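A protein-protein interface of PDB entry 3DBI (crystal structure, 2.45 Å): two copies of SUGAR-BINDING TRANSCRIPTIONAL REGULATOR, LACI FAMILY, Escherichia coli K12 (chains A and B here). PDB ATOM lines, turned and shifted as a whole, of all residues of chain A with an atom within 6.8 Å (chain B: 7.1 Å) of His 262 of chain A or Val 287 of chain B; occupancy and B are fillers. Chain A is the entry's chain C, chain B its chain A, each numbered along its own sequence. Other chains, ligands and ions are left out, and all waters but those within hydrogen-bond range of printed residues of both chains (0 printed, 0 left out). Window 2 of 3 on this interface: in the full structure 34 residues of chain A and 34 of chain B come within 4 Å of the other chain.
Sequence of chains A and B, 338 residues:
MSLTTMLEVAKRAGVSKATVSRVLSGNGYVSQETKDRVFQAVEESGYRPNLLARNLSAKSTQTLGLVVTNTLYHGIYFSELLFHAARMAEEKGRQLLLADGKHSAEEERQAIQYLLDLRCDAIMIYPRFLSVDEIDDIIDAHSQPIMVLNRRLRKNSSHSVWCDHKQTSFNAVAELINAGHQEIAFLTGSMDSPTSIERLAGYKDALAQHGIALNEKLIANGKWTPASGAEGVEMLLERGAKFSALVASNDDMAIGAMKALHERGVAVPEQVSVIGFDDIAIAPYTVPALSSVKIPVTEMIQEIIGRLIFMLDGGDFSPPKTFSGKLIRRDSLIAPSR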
ATOM      1  N   VAL A 233       3.585  22.344 -40.340  1.00  0.00           N
ATOM      2  CA  VAL A 233       4.154  23.207 -39.306  1.00  0.00           C
ATOM      3  C   VAL A 233       5.632  22.865 -39.079  1.00  0.00           C
ATOM      4  O   VAL A 233       6.477  23.757 -38.967  1.00  0.00           O
ATOM      5  CB  VAL A 233       3.317  23.132 -37.993  1.00  0.00           C
ATOM      6  CG1 VAL A 233       4.142  23.478 -36.751  1.00  0.00           C
ATOM      7  CG2 VAL A 233       2.132  24.052 -38.098  1.00  0.00           C
ATOM      8  N   ILE A 255      -6.021  21.077 -37.046  1.00  0.00           N
ATOM      9  CA  ILE A 255      -5.917  20.437 -35.739  1.00  0.00           C
ATOM     10  C   ILE A 255      -4.540  19.785 -35.593  1.00  0.00           C
ATOM     11  O   ILE A 255      -3.892  19.905 -34.547  1.00  0.00           O
ATOM     12  CB  ILE A 255      -7.097  19.454 -35.479  1.00  0.00           C
ATOM     13  CG1 ILE A 255      -8.409  20.239 -35.325  1.00  0.00           C
ATOM     14  CG2 ILE A 255      -6.861  18.614 -34.224  1.00  0.00           C
ATOM     15  CD1 ILE A 255      -9.686  19.397 -35.399  1.00  0.00           C
ATOM     16  N   ALA A 257      -1.852  20.835 -37.295  1.00  0.00           N
ATOM     17  CA  ALA A 257      -1.024  22.031 -37.151  1.00  0.00           C
ATOM     18  C   ALA A 257      -0.962  22.506 -35.703  1.00  0.00           C
ATOM     19  O   ALA A 257       0.126  22.668 -35.161  1.00  0.00           O
ATOM     20  CB  ALA A 257      -1.521  23.139 -38.048  1.00  0.00           C
ATOM     21  N   MET A 258      -2.123  22.679 -35.073  1.00  0.00           N
ATOM     22  CA  MET A 258      -2.198  23.133 -33.675  1.00  0.00           C
ATOM     23  C   MET A 258      -1.473  22.207 -32.704  1.00  0.00           C
ATOM     24  O   MET A 258      -0.824  22.671 -31.775  1.00  0.00           O
ATOM     25  CB  MET A 258      -3.648  23.357 -33.230  1.00  0.00           C
ATOM     26  CG  MET A 258      -4.275  24.602 -33.845  1.00  0.00           C
ATOM     27  SD  MET A 258      -6.032  25.062 -33.133  1.00  0.00           S
ATOM     28  CE  MET A 258      -6.967  23.395 -33.465  1.00  0.00           C
ATOM     29  N   LYS A 259      -1.566  20.906 -32.954  1.00  0.00           N
ATOM     30  CA  LYS A 259      -0.892  19.892 -32.159  1.00  0.00           C
ATOM     31  C   LYS A 259       0.628  20.027 -32.249  1.00  0.00           C
ATOM     32  O   LYS A 259       1.324  19.940 -31.236  1.00  0.00           O
ATOM     33  CB  LYS A 259      -1.337  18.497 -32.617  1.00  0.00           C
ATOM     34  CG  LYS A 259      -0.617  17.317 -31.963  1.00  0.00           C
ATOM     35  CD  LYS A 259      -0.970  17.155 -30.490  1.00  0.00           C
ATOM     36  CE  LYS A 259      -0.368  15.881 -29.929  1.00  0.00           C
ATOM     37  NZ  LYS A 259      -0.739  15.679 -28.506  1.00  0.00           N
ATOM     38  N   ALA A 260       1.129  20.255 -33.458  1.00  0.00           N
ATOM     39  CA  ALA A 260       2.562  20.404 -33.678  1.00  0.00           C
ATOM     40  C   ALA A 260       3.083  21.716 -33.102  1.00  0.00           C
ATOM     41  O   ALA A 260       4.171  21.750 -32.530  1.00  0.00           O
ATOM     42  CB  ALA A 260       2.889  20.292 -35.149  1.00  0.00           C
ATOM     43  N   LEU A 261       2.289  22.777 -33.239  1.00  0.00           N
ATOM     44  CA  LEU A 261       2.594  24.069 -32.621  1.00  0.00           C
ATOM     45  C   LEU A 261       2.628  23.984 -31.095  1.00  0.00           C
ATOM     46  O   LEU A 261       3.503  24.584 -30.466  1.00  0.00           O
ATOM     47  CB  LEU A 261       1.611  25.145 -33.081  1.00  0.00           C
ATOM     48  CG  LEU A 261       1.760  25.641 -34.523  1.00  0.00           C
ATOM     49  CD1 LEU A 261       0.501  26.356 -34.982  1.00  0.00           C
ATOM     50  CD2 LEU A 261       2.967  26.543 -34.687  1.00  0.00           C
ATOM     51  N   HIS A 262       1.705  23.220 -30.510  1.00  0.00           N
ATOM     52  CA  HIS A 262       1.702  23.007 -29.062  1.00  0.00           C
ATOM     53  C   HIS A 262       2.947  22.269 -28.580  1.00  0.00           C
ATOM     54  O   HIS A 262       3.550  22.642 -27.570  1.00  0.00           O
ATOM     55  CB  HIS A 262       0.449  22.266 -28.583  1.00  0.00           C
ATOM     56  CG  HIS A 262       0.479  21.937 -27.119  1.00  0.00           C
ATOM     57  ND1 HIS A 262       0.252  22.883 -26.139  1.00  0.00           N
ATOM     58  CD2 HIS A 262       0.752  20.780 -26.469  1.00  0.00           C
ATOM     59  CE1 HIS A 262       0.361  22.317 -24.950  1.00  0.00           C
ATOM     60  NE2 HIS A 262       0.666  21.042 -25.122  1.00  0.00           N
ATOM     61  N   GLU A 263       3.326  21.227 -29.315  1.00  0.00           N
ATOM     62  CA  GLU A 263       4.468  20.389 -28.949  1.00  0.00           C
ATOM     63  C   GLU A 263       5.818  21.074 -29.161  1.00  0.00           C
ATOM     64  O   GLU A 263       6.838  20.601 -28.671  1.00  0.00           O
ATOM     65  CB  GLU A 263       4.420  19.063 -29.702  1.00  0.00           C
ATOM     66  CG  GLU A 263       3.404  18.097 -29.136  1.00  0.00           C
ATOM     67  CD  GLU A 263       3.478  16.717 -29.768  1.00  0.00           C
ATOM     68  OE1 GLU A 263       3.567  16.623 -31.013  1.00  0.00           O
ATOM     69  OE2 GLU A 263       3.433  15.722 -29.012  1.00  0.00           O
ATOM     70  N   ARG A 264       5.810  22.189 -29.886  1.00  0.00           N
ATOM     71  CA  ARG A 264       7.018  22.984 -30.083  1.00  0.00           C
ATOM     72  C   ARG A 264       6.950  24.301 -29.317  1.00  0.00           C
ATOM     73  O   ARG A 264       7.649  25.259 -29.646  1.00  0.00           O
ATOM     74  CB  ARG A 264       7.244  23.253 -31.572  1.00  0.00           C
ATOM     75  CG  ARG A 264       7.516  22.004 -32.395  1.00  0.00           C
ATOM     76  CD  ARG A 264       8.956  21.542 -32.235  1.00  0.00           C
ATOM     77  NE  ARG A 264       9.857  22.230 -33.155  1.00  0.00           N
ATOM     78  CZ  ARG A 264      10.706  21.613 -33.969  1.00  0.00           C
ATOM     79  NH1 ARG A 264      10.774  20.289 -33.982  1.00  0.00           N
ATOM     80  NH2 ARG A 264      11.490  22.321 -34.772  1.00  0.00           N
ATOM     81  N   GLY A 265       6.102  24.340 -28.294  1.00  0.00           N
ATOM     82  CA  GLY A 265       6.037  25.484 -27.383  1.00  0.00           C
ATOM     83  C   GLY A 265       5.538  26.786 -27.991  1.00  0.00           C
ATOM     84  O   GLY A 265       5.755  27.855 -27.426  1.00  0.00           O
ATOM     85  N   VAL A 266       4.866  26.699 -29.136  1.00  0.00           N
ATOM     86  CA  VAL A 266       4.270  27.873 -29.778  1.00  0.00           C
ATOM     87  C   VAL A 266       2.800  28.025 -29.389  1.00  0.00           C
ATOM     88  O   VAL A 266       1.980  27.136 -29.643  1.00  0.00           O
ATOM     89  CB  VAL A 266       4.414  27.830 -31.318  1.00  0.00           C
ATOM     90  CG1 VAL A 266       3.832  29.081 -31.938  1.00  0.00           C
ATOM     91  CG2 VAL A 266       5.878  27.687 -31.717  1.00  0.00           C
ATOM     92  N   ALA A 267       2.479  29.163 -28.780  1.00  0.00           N
ATOM     93  CA  ALA A 267       1.150  29.422 -28.241  1.00  0.00           C
ATOM     94  C   ALA A 267       0.139  29.770 -29.325  1.00  0.00           C
ATOM     95  O   ALA A 267       0.383  30.622 -30.178  1.00  0.00           O
ATOM     96  CB  ALA A 267       1.209  30.529 -27.188  1.00  0.00           C
ATOM     97  N   VAL A 268      -0.993  29.080 -29.283  1.00  0.00           N
ATOM     98  CA  VAL A 268      -2.141  29.401 -30.123  1.00  0.00           C
ATOM     99  C   VAL A 268      -3.255  29.920 -29.197  1.00  0.00           C
ATOM    100  O   VAL A 268      -3.599  29.255 -28.218  1.00  0.00           O
ATOM    101  CB  VAL A 268      -2.605  28.148 -30.927  1.00  0.00           C
ATOM    102  CG1 VAL A 268      -3.835  28.448 -31.790  1.00  0.00           C
ATOM    103  CG2 VAL A 268      -1.467  27.614 -31.792  1.00  0.00           C
ATOM    104  N   VAL A 287      -8.865  23.001 -28.321  1.00  0.00           N
ATOM    105  CA  VAL A 287      -8.255  23.959 -27.411  1.00  0.00           C
ATOM    106  C   VAL A 287      -7.091  24.673 -28.101  1.00  0.00           C
ATOM    107  O   VAL A 287      -6.034  24.072 -28.286  1.00  0.00           O
ATOM    108  CB  VAL A 287      -7.728  23.302 -26.117  1.00  0.00           C
ATOM    109  CG1 VAL A 287      -7.447  24.372 -25.069  1.00  0.00           C
ATOM    110  CG2 VAL A 287      -8.689  22.242 -25.582  1.00  0.00           C
ATOM    111  N   MET B 258     -13.476  16.743 -22.877  1.00  0.00           N
ATOM    112  CA  MET B 258     -12.156  17.333 -22.607  1.00  0.00           C
ATOM    113  C   MET B 258     -12.142  18.859 -22.675  1.00  0.00           C
ATOM    114  O   MET B 258     -11.411  19.498 -21.928  1.00  0.00           O
ATOM    115  CB  MET B 258     -11.086  16.760 -23.533  1.00  0.00           C
ATOM    116  CG  MET B 258     -10.643  15.349 -23.168  1.00  0.00           C
ATOM    117  SD  MET B 258      -9.154  14.648 -24.224  1.00  0.00           S
ATOM    118  CE  MET B 258      -9.854  14.932 -26.015  1.00  0.00           C
ATOM    119  N   HIS B 262     -11.328  21.220 -19.457  1.00  0.00           N
ATOM    120  CA  HIS B 262     -10.308  22.263 -19.571  1.00  0.00           C
ATOM    121  C   HIS B 262     -10.834  23.649 -19.188  1.00  0.00           C
ATOM    122  O   HIS B 262     -10.130  24.420 -18.533  1.00  0.00           O
ATOM    123  CB  HIS B 262      -9.718  22.289 -20.985  1.00  0.00           C
ATOM    124  CG  HIS B 262      -8.719  23.383 -21.205  1.00  0.00           C
ATOM    125  ND1 HIS B 262      -7.402  23.279 -20.809  1.00  0.00           N
ATOM    126  CD2 HIS B 262      -8.846  24.607 -21.775  1.00  0.00           C
ATOM    127  CE1 HIS B 262      -6.760  24.390 -21.128  1.00  0.00           C
ATOM    128  NE2 HIS B 262      -7.613  25.211 -21.715  1.00  0.00           N
ATOM    129  N   VAL B 268      -6.460  17.259 -17.697  1.00  0.00           N
ATOM    130  CA  VAL B 268      -6.479  15.970 -18.377  1.00  0.00           C
ATOM    131  C   VAL B 268      -5.067  15.720 -18.913  1.00  0.00           C
ATOM    132  O   VAL B 268      -4.539  16.548 -19.661  1.00  0.00           O
ATOM    133  CB  VAL B 268      -7.519  15.950 -19.535  1.00  0.00           C
ATOM    134  CG1 VAL B 268      -7.457  14.640 -20.321  1.00  0.00           C
ATOM    135  CG2 VAL B 268      -8.928  16.175 -18.997  1.00  0.00           C
ATOM    136  N   ILE B 282      -8.587  12.136 -36.023  1.00  0.00           N
ATOM    137  CA  ILE B 282      -8.264  13.323 -35.247  1.00  0.00           C
ATOM    138  C   ILE B 282      -7.640  12.972 -33.883  1.00  0.00           C
ATOM    139  O   ILE B 282      -6.873  13.761 -33.323  1.00  0.00           O
ATOM    140  CB  ILE B 282      -9.552  14.231 -35.146  1.00  0.00           C
ATOM    141  CG1 ILE B 282      -9.574  15.267 -36.276  1.00  0.00           C
ATOM    142  CG2 ILE B 282      -9.755  14.872 -33.780  1.00  0.00           C
ATOM    143  CD1 ILE B 282      -8.251  15.963 -36.503  1.00  0.00           C
ATOM    144  N   ALA B 283      -7.936  11.775 -33.378  1.00  0.00           N
ATOM    145  CA  ALA B 283      -7.608  11.407 -31.995  1.00  0.00           C
ATOM    146  C   ALA B 283      -6.156  11.622 -31.507  1.00  0.00           C
ATOM    147  O   ALA B 283      -5.968  12.162 -30.407  1.00  0.00           O
ATOM    148  CB  ALA B 283      -8.091   9.987 -31.673  1.00  0.00           C
ATOM    149  N   PRO B 284      -5.130  11.226 -32.310  1.00  0.00           N
ATOM    150  CA  PRO B 284      -3.766  11.464 -31.822  1.00  0.00           C
ATOM    151  C   PRO B 284      -3.341  12.927 -31.841  1.00  0.00           C
ATOM    152  O   PRO B 284      -2.276  13.255 -31.321  1.00  0.00           O
ATOM    153  CB  PRO B 284      -2.891  10.661 -32.801  1.00  0.00           C
ATOM    154  CG  PRO B 284      -3.844   9.772 -33.560  1.00  0.00           C
ATOM    155  CD  PRO B 284      -5.105  10.549 -33.621  1.00  0.00           C
ATOM    156  N   TYR B 285      -4.176  13.797 -32.401  1.00  0.00           N
ATOM    157  CA  TYR B 285      -3.832  15.205 -32.577  1.00  0.00           C
ATOM    158  C   TYR B 285      -4.566  16.146 -31.633  1.00  0.00           C
ATOM    159  O   TYR B 285      -4.453  17.367 -31.760  1.00  0.00           O
ATOM    160  CB  TYR B 285      -4.024  15.597 -34.040  1.00  0.00           C
ATOM    161  CG  TYR B 285      -3.175  14.736 -34.930  1.00  0.00           C
ATOM    162  CD1 TYR B 285      -1.840  15.063 -35.177  1.00  0.00           C
ATOM    163  CD2 TYR B 285      -3.679  13.552 -35.469  1.00  0.00           C
ATOM    164  CE1 TYR B 285      -1.042  14.248 -35.971  1.00  0.00           C
ATOM    165  CE2 TYR B 285      -2.895  12.733 -36.259  1.00  0.00           C
ATOM    166  CZ  TYR B 285      -1.585  13.086 -36.511  1.00  0.00           C
ATOM    167  OH  TYR B 285      -0.836  12.253 -37.295  1.00  0.00           O
ATOM    168  N   THR B 286      -5.313  15.579 -30.685  1.00  0.00           N
ATOM    169  CA  THR B 286      -5.949  16.379 -29.640  1.00  0.00           C
ATOM    170  C   THR B 286      -4.921  16.628 -28.541  1.00  0.00           C
ATOM    171  O   THR B 286      -3.875  15.981 -28.518  1.00  0.00           O
ATOM    172  CB  THR B 286      -7.211  15.702 -29.050  1.00  0.00           C
ATOM    173  OG1 THR B 286      -6.871  14.411 -28.545  1.00  0.00           O
ATOM    174  CG2 THR B 286      -8.299  15.563 -30.099  1.00  0.00           C
ATOM    175  N   VAL B 287      -5.212  17.581 -27.655  1.00  0.00           N
ATOM    176  CA  VAL B 287      -4.334  17.909 -26.529  1.00  0.00           C
ATOM    177  C   VAL B 287      -5.057  17.614 -25.210  1.00  0.00           C
ATOM    178  O   VAL B 287      -5.930  18.378 -24.811  1.00  0.00           O
ATOM    179  CB  VAL B 287      -3.945  19.403 -26.508  1.00  0.00           C
ATOM    180  CG1 VAL B 287      -2.713  19.623 -25.630  1.00  0.00           C
ATOM    181  CG2 VAL B 287      -3.755  19.968 -27.917  1.00  0.00           C
ATOM    182  N   PRO B 288      -4.705  16.509 -24.528  1.00  0.00           N
ATOM    183  CA  PRO B 288      -3.742  15.475 -24.919  1.00  0.00           C
ATOM    184  C   PRO B 288      -4.338  14.475 -25.911  1.00  0.00           C
ATOM    185  O   PRO B 288      -5.556  14.474 -26.147  1.00  0.00           O
ATOM    186  CB  PRO B 288      -3.441  14.770 -23.598  1.00  0.00           C
ATOM    187  CG  PRO B 288      -4.690  14.887 -22.833  1.00  0.00           C
ATOM    188  CD  PRO B 288      -5.301  16.217 -23.210  1.00  0.00           C
ATOM    189  N   ALA B 289      -3.470  13.654 -26.494  1.00  0.00           N
ATOM    190  CA  ALA B 289      -3.850  12.700 -27.525  1.00  0.00           C
ATOM    191  C   ALA B 289      -4.887  11.714 -26.992  1.00  0.00           C
ATOM    192  O   ALA B 289      -4.676  11.079 -25.957  1.00  0.00           O
ATOM    193  CB  ALA B 289      -2.621  11.978 -28.037  1.00  0.00           C
ATOM    194  N   LEU B 290      -6.013  11.611 -27.691  1.00  0.00           N
ATOM    195  CA  LEU B 290      -7.160  10.871 -27.179  1.00  0.00           C
ATOM    196  C   LEU B 290      -7.012   9.355 -27.271  1.00  0.00           C
ATOM    197  O   LEU B 290      -6.911   8.799 -28.369  1.00  0.00           O
ATOM    198  CB  LEU B 290      -8.458  11.323 -27.866  1.00  0.00           C
ATOM    199  CG  LEU B 290      -9.740  10.582 -27.448  1.00  0.00           C
ATOM    200  CD1 LEU B 290     -10.064  10.776 -25.962  1.00  0.00           C
ATOM    201  CD2 LEU B 290     -10.928  10.988 -28.319  1.00  0.00           C
ATOM    202  N   SER B 332      -3.987  10.631 -23.056  1.00  0.00           N
ATOM    203  CA  SER B 332      -5.157  10.981 -22.241  1.00  0.00           C
ATOM    204  C   SER B 332      -5.428  10.012 -21.078  1.00  0.00           C
ATOM    205  O   SER B 332      -6.237  10.312 -20.200  1.00  0.00           O
ATOM    206  CB  SER B 332      -6.409  11.132 -23.117  1.00  0.00           C
ATOM    207  OG  SER B 332      -6.939   9.869 -23.494  1.00  0.00           O
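The side-chain amino group (NZ) of Lys 259 of chain A lies within hydrogen-bond range of the backbone carbonyl oxygen (O) of Thr 286 of chain B (3.2 Å).
O of Ala 283 of chain B lies within hydrogen-bond range of OG1 of Thr 286 of chain B (3.1 Å).
OG1 of Thr 286 of chain B lies within hydrogen-bond range of O of Pro 288 of chain B.
The backbone NH (N) of Leu 290 of chain B lies within hydrogen-bond range of the side-chain hydroxyl (OG1) of Thr 286 of chain B.
O of Ala 289 of chain B sits at hydrogen-bond distance from N of Ser 332 of chain B (3.0 Å).
Among the printed residues, pairs that only touch across the chains: Ile 255 of chain A with Ile 282 of chain B (3.8 Å), Ile 255 of chain A with Tyr 285 of chain B (3.7 Å), Lys 259 of chain A with Pro 284 of chain B (3.5 Å), Lys 259 of chain A with Tyr 285 of chain B (3.4 Å), Lys 259 of chain A with Ala 289 of chain B (3.95 Å), His 262 of chain A with Val 287 of chain B (3.7 Å) and Val 287 of chain A with His 262 of chain B (3.5 Å).
Of the printed residues of chain B, Ile 255 of chain A touches Ile 282 and Tyr 285.
Met 258 of chain A touches none of the printed residues of chain B.
Printed residues of chain B within 4 Å of His 262 of chain A: Val 287 (3.7 Å).
Gly 265 of chain A touches none of the printed residues of chain B.
Of the printed residues of chain B, Val 287 of chain A touches His 262.
Of the printed residues of chain A, His 262 of chain B touches Val 287 (3.5 Å).
Printed residues of chain A within 4 Å of Ile 282 of chain B: Ile 255.
Of the printed residues of chain A, Pro 284 of chain B touches Lys 259.
Val 287 of chain B touches one residue of chain A.
The nearest residue of chain B that does not touch His 262 of chain A is Thr 286 of chain B (7.0 Å).
Printed residues of chain A that touch a printed residue of chain B: Ile 255, Lys 259, His 262 and Val 287.
Hydrophobic or aromatic side chains of chain A that line the printed part of chain B: Ile 255, His 262 and Val 287.
Along chain A the printed residues that touch a printed residue of chain B span positions 255 to 287.
Among the printed residues, 8 pairs touch across the chains.
Among the printed residues, no Asp or Glu carboxylate lies within 4 Å of a Lys or Arg side-chain nitrogen of the other chain.
His 262 of chain A touches Val 287 of chain B, and with the chains exchanged Val 287 of chain A touches His 262 of chain B.
Positions printed for both chains: 258, 262, 268 and 287.
Of the 8 pairs that touch across the chains among the printed residues, 2 have their exchanged pair printed and touching as well.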
